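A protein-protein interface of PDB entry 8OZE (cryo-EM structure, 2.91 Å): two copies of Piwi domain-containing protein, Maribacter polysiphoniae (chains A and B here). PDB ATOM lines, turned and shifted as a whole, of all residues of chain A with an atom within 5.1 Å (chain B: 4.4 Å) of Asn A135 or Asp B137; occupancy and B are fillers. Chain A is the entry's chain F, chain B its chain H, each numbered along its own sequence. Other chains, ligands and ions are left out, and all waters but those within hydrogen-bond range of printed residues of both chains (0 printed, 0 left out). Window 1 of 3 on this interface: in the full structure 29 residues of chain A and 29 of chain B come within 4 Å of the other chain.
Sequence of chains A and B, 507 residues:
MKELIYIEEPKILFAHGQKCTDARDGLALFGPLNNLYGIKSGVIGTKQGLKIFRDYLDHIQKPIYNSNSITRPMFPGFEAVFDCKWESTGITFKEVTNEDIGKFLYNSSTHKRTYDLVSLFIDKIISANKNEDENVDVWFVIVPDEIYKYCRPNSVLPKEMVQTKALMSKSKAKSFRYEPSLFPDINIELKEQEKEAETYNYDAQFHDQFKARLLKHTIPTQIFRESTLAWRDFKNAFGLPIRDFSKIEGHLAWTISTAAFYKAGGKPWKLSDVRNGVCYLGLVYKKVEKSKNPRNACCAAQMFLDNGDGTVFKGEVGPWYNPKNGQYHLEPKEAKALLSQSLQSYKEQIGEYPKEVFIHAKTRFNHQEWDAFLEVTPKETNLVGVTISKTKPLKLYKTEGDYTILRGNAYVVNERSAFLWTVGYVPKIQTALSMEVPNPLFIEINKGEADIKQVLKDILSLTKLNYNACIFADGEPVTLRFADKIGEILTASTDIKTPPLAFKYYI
The side-chain carboxylate (OD2) of Asp B137 is in salt-bridge range of the side-chain amino group (NZ) of Lys A40 (3.8 Å).
OD1 of Asp B137 lies within hydrogen-bond range of ND2 of Asn A135 (3.0 Å).
ND2 of Asn A135 lies within hydrogen-bond range of O of Ala B264 (2.9 Å).
The side-chain carboxylate (OD2) of Asp A137 is in salt-bridge range of the side-chain amino group (NZ) of Lys B40 (3.8 Å).
The side-chain carboxylate (OD1) of Asp A137 is in hydrogen-bond range of the side-chain amide nitrogen (ND2) of Asn B135 (3.0 Å).
Asn A135 touches just these residues of chain B: Asp B137 and Ala B264.
Printed residues of chain A within 4 Å of Gly B265: Asp A133.
Printed residues of chain B within 4 Å of Asp A133: Gly B265 (3.3 Å).
Printed residues of chain B within 4 Å of Asp A137: Lys B40 and Asn B135.
Printed residues of chain A within 4 Å of Lys B40: Asp A137 (3.8 Å).
Val B136 touches none of the printed residues of chain A.
The nearest residue of chain B that does not touch Asn A135 is Gly B265 (4.03 Å).
The nearest printed residue of chain B that does not touch Lys A40 is Gly B265 (5.6 Å).
N of Asp A137 is in hydrogen-bond range of O of Lys A40 (2.7 Å).
O of Lys B40 sits at hydrogen-bond distance from N of Asp B137.
Of the 11 printed residues of chain B, 6 touch a printed residue of chain A.
Printed residues of chain B that touch a printed residue of chain A: Gly B38, Lys B40, Asn B135, Asp B137, Ala B264 and Gly B265.
Among the printed residues, 8 pairs touch across the chains.
Among the printed residues, Asp or Glu carboxylates within 4 Å of a Lys or Arg side-chain nitrogen of the other chain: Lys A40 with Asp B137 and Asp A137 with Lys B40.
Lys A40 touches Gly B38.
Ala B264 touches Lys A40 (O to NZ, 3.6 Å).
CA of Gly B265 touches O of Asp A133, at 3.3 Å.
Lys A40 touches Asp B137, and with the chains exchanged Asp A137 touches Lys B40.
Asn A135 touches Asp B137, and with the chains exchanged Asp A137 touches Asn B135.
Of the 8 pairs that touch across the chains among the printed residues, 4 have their exchanged pair printed and touching as well.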
ATOM      1  N   LYS A  40     -31.077   8.453   0.993  1.00  0.00           N
ATOM      2  CA  LYS A  40     -31.258   7.967   2.355  1.00  0.00           C
ATOM      3  C   LYS A  40     -32.274   8.873   3.037  1.00  0.00           C
ATOM      4  O   LYS A  40     -32.023  10.066   3.226  1.00  0.00           O
ATOM      5  CB  LYS A  40     -29.927   7.953   3.098  1.00  0.00           C
ATOM      6  CG  LYS A  40     -28.793   7.355   2.291  1.00  0.00           C
ATOM      7  CD  LYS A  40     -27.445   7.674   2.902  1.00  0.00           C
ATOM      8  CE  LYS A  40     -26.321   7.403   1.918  1.00  0.00           C
ATOM      9  NZ  LYS A  40     -24.998   7.806   2.469  1.00  0.00           N
ATOM     10  N   ASP A 133     -25.015   8.929  13.803  1.00  0.00           N
ATOM     11  CA  ASP A 133     -24.083   8.581  12.738  1.00  0.00           C
ATOM     12  C   ASP A 133     -24.782   8.306  11.413  1.00  0.00           C
ATOM     13  O   ASP A 133     -24.118   8.251  10.374  1.00  0.00           O
ATOM     14  CB  ASP A 133     -23.251   7.366  13.152  1.00  0.00           C
ATOM     15  CG  ASP A 133     -22.263   7.687  14.253  1.00  0.00           C
ATOM     16  OD1 ASP A 133     -21.351   8.505  14.013  1.00  0.00           O
ATOM     17  OD2 ASP A 133     -22.399   7.127  15.361  1.00  0.00           O
ATOM     18  N   GLU A 134     -26.101   8.129  11.422  1.00  0.00           N
ATOM     19  CA  GLU A 134     -26.821   7.895  10.179  1.00  0.00           C
ATOM     20  C   GLU A 134     -26.760   9.123   9.279  1.00  0.00           C
ATOM     21  O   GLU A 134     -26.777  10.266   9.742  1.00  0.00           O
ATOM     22  CB  GLU A 134     -28.280   7.530  10.459  1.00  0.00           C
ATOM     23  CG  GLU A 134     -28.485   6.169  11.102  1.00  0.00           C
ATOM     24  CD  GLU A 134     -28.297   6.192  12.605  1.00  0.00           C
ATOM     25  OE1 GLU A 134     -28.051   7.281  13.162  1.00  0.00           O
ATOM     26  OE2 GLU A 134     -28.403   5.117  13.232  1.00  0.00           O
ATOM     27  N   ASN A 135     -26.687   8.873   7.978  1.00  0.00           N
ATOM     28  CA  ASN A 135     -26.693   9.923   6.970  1.00  0.00           C
ATOM     29  C   ASN A 135     -28.050   9.935   6.281  1.00  0.00           C
ATOM     30  O   ASN A 135     -28.535   8.889   5.837  1.00  0.00           O
ATOM     31  CB  ASN A 135     -25.575   9.702   5.949  1.00  0.00           C
ATOM     32  CG  ASN A 135     -25.364  10.895   5.038  1.00  0.00           C
ATOM     33  OD1 ASN A 135     -26.293  11.643   4.740  1.00  0.00           O
ATOM     34  ND2 ASN A 135     -24.131  11.076   4.585  1.00  0.00           N
ATOM     35  N   VAL A 136     -28.663  11.112   6.205  1.00  0.00           N
ATOM     36  CA  VAL A 136     -29.970  11.285   5.585  1.00  0.00           C
ATOM     37  C   VAL A 136     -29.879  12.420   4.576  1.00  0.00           C
ATOM     38  O   VAL A 136     -29.287  13.466   4.864  1.00  0.00           O
ATOM     39  CB  VAL A 136     -31.073  11.559   6.622  1.00  0.00           C
ATOM     40  CG1 VAL A 136     -31.234  10.369   7.546  1.00  0.00           C
ATOM     41  CG2 VAL A 136     -30.739  12.795   7.432  1.00  0.00           C
ATOM     42  N   ASP A 137     -30.429  12.200   3.383  1.00  0.00           N
ATOM     43  CA  ASP A 137     -30.466  13.265   2.390  1.00  0.00           C
ATOM     44  C   ASP A 137     -31.678  14.165   2.591  1.00  0.00           C
ATOM     45  O   ASP A 137     -31.556  15.394   2.558  1.00  0.00           O
ATOM     46  CB  ASP A 137     -30.462  12.672   0.983  1.00  0.00           C
ATOM     47  CG  ASP A 137     -29.187  11.920   0.674  1.00  0.00           C
ATOM     48  OD1 ASP A 137     -28.116  12.345   1.154  1.00  0.00           O
ATOM     49  OD2 ASP A 137     -29.251  10.907  -0.051  1.00  0.00           O
ATOM     50  N   GLY B  38     -24.097   5.034  -1.993  1.00  0.00           N
ATOM     51  CA  GLY B  38     -22.940   5.665  -2.593  1.00  0.00           C
ATOM     52  C   GLY B  38     -22.425   6.788  -1.727  1.00  0.00           C
ATOM     53  O   GLY B  38     -23.147   7.336  -0.889  1.00  0.00           O
ATOM     54  N   ILE B  39     -21.158   7.125  -1.943  1.00  0.00           N
ATOM     55  CA  ILE B  39     -20.500   8.221  -1.244  1.00  0.00           C
ATOM     56  C   ILE B  39     -20.239   9.320  -2.261  1.00  0.00           C
ATOM     57  O   ILE B  39     -19.445   9.143  -3.191  1.00  0.00           O
ATOM     58  CB  ILE B  39     -19.199   7.775  -0.569  1.00  0.00           C
ATOM     59  CG1 ILE B  39     -19.487   6.722   0.498  1.00  0.00           C
ATOM     60  CG2 ILE B  39     -18.488   8.968   0.050  1.00  0.00           C
ATOM     61  CD1 ILE B  39     -18.252   6.201   1.177  1.00  0.00           C
ATOM     62  N   LYS B  40     -20.910  10.454  -2.087  1.00  0.00           N
ATOM     63  CA  LYS B  40     -20.709  11.621  -2.936  1.00  0.00           C
ATOM     64  C   LYS B  40     -19.637  12.485  -2.288  1.00  0.00           C
ATOM     65  O   LYS B  40     -19.835  13.006  -1.187  1.00  0.00           O
ATOM     66  CB  LYS B  40     -22.016  12.384  -3.116  1.00  0.00           C
ATOM     67  CG  LYS B  40     -23.197  11.488  -3.433  1.00  0.00           C
ATOM     68  CD  LYS B  40     -24.512  12.218  -3.256  1.00  0.00           C
ATOM     69  CE  LYS B  40     -25.676  11.243  -3.210  1.00  0.00           C
ATOM     70  NZ  LYS B  40     -26.963  11.935  -2.936  1.00  0.00           N
ATOM     71  N   ASN B 135     -25.070  17.453  -3.489  1.00  0.00           N
ATOM     72  CA  ASN B 135     -25.052  16.774  -2.201  1.00  0.00           C
ATOM     73  C   ASN B 135     -23.716  16.063  -2.040  1.00  0.00           C
ATOM     74  O   ASN B 135     -23.287  15.329  -2.936  1.00  0.00           O
ATOM     75  CB  ASN B 135     -26.208  15.778  -2.097  1.00  0.00           C
ATOM     76  CG  ASN B 135     -26.399  15.240  -0.692  1.00  0.00           C
ATOM     77  OD1 ASN B 135     -25.450  15.124   0.081  1.00  0.00           O
ATOM     78  ND2 ASN B 135     -27.636  14.904  -0.357  1.00  0.00           N
ATOM     79  N   VAL B 136     -23.060  16.290  -0.907  1.00  0.00           N
ATOM     80  CA  VAL B 136     -21.765  15.690  -0.609  1.00  0.00           C
ATOM     81  C   VAL B 136     -21.843  15.038   0.764  1.00  0.00           C
ATOM     82  O   VAL B 136     -22.384  15.627   1.708  1.00  0.00           O
ATOM     83  CB  VAL B 136     -20.623  16.716  -0.664  1.00  0.00           C
ATOM     84  CG1 VAL B 136     -20.482  17.271  -2.069  1.00  0.00           C
ATOM     85  CG2 VAL B 136     -20.883  17.850   0.307  1.00  0.00           C
ATOM     86  N   ASP B 137     -21.336  13.810   0.867  1.00  0.00           N
ATOM     87  CA  ASP B 137     -21.287  13.148   2.164  1.00  0.00           C
ATOM     88  C   ASP B 137     -20.036  13.542   2.937  1.00  0.00           C
ATOM     89  O   ASP B 137     -20.110  13.854   4.130  1.00  0.00           O
ATOM     90  CB  ASP B 137     -21.356  11.634   1.985  1.00  0.00           C
ATOM     91  CG  ASP B 137     -22.670  11.181   1.387  1.00  0.00           C
ATOM     92  OD1 ASP B 137     -23.708  11.801   1.694  1.00  0.00           O
ATOM     93  OD2 ASP B 137     -22.668  10.203   0.613  1.00  0.00           O
ATOM     94  N   VAL B 138     -18.879  13.536   2.277  1.00  0.00           N
ATOM     95  CA  VAL B 138     -17.605  13.843   2.915  1.00  0.00           C
ATOM     96  C   VAL B 138     -16.856  14.852   2.056  1.00  0.00           C
ATOM     97  O   VAL B 138     -16.839  14.743   0.826  1.00  0.00           O
ATOM     98  CB  VAL B 138     -16.755  12.573   3.125  1.00  0.00           C
ATOM     99  CG1 VAL B 138     -15.515  12.889   3.939  1.00  0.00           C
ATOM    100  CG2 VAL B 138     -17.571  11.484   3.793  1.00  0.00           C
ATOM    101  N   PRO B 220     -18.700  16.445   7.550  1.00  0.00           N
ATOM    102  CA  PRO B 220     -17.607  15.475   7.702  1.00  0.00           C
ATOM    103  C   PRO B 220     -16.520  15.724   6.667  1.00  0.00           C
ATOM    104  O   PRO B 220     -16.782  15.741   5.464  1.00  0.00           O
ATOM    105  CB  PRO B 220     -18.295  14.122   7.483  1.00  0.00           C
ATOM    106  CG  PRO B 220     -19.762  14.399   7.588  1.00  0.00           C
ATOM    107  CD  PRO B 220     -19.942  15.797   7.106  1.00  0.00           C
ATOM    108  N   LYS B 263     -17.159   8.213   7.719  1.00  0.00           N
ATOM    109  CA  LYS B 263     -17.557   9.612   7.650  1.00  0.00           C
ATOM    110  C   LYS B 263     -18.821   9.821   6.830  1.00  0.00           C
ATOM    111  O   LYS B 263     -19.534  10.803   7.055  1.00  0.00           O
ATOM    112  CB  LYS B 263     -16.419  10.446   7.070  1.00  0.00           C
ATOM    113  CG  LYS B 263     -15.379  10.849   8.084  1.00  0.00           C
ATOM    114  CD  LYS B 263     -14.056  11.132   7.414  1.00  0.00           C
ATOM    115  CE  LYS B 263     -13.007  11.488   8.439  1.00  0.00           C
ATOM    116  NZ  LYS B 263     -13.397  12.699   9.203  1.00  0.00           N
ATOM    117  N   ALA B 264     -19.115   8.930   5.889  1.00  0.00           N
ATOM    118  CA  ALA B 264     -20.288   9.060   5.038  1.00  0.00           C
ATOM    119  C   ALA B 264     -21.557   8.533   5.690  1.00  0.00           C
ATOM    120  O   ALA B 264     -22.634   8.663   5.104  1.00  0.00           O
ATOM    121  CB  ALA B 264     -20.058   8.337   3.710  1.00  0.00           C
ATOM    122  N   GLY B 265     -21.460   7.944   6.876  1.00  0.00           N
ATOM    123  CA  GLY B 265     -22.637   7.460   7.567  1.00  0.00           C
ATOM    124  C   GLY B 265     -22.802   5.958   7.497  1.00  0.00           C
ATOM    125  O   GLY B 265     -23.926   5.454   7.428  1.00  0.00           O
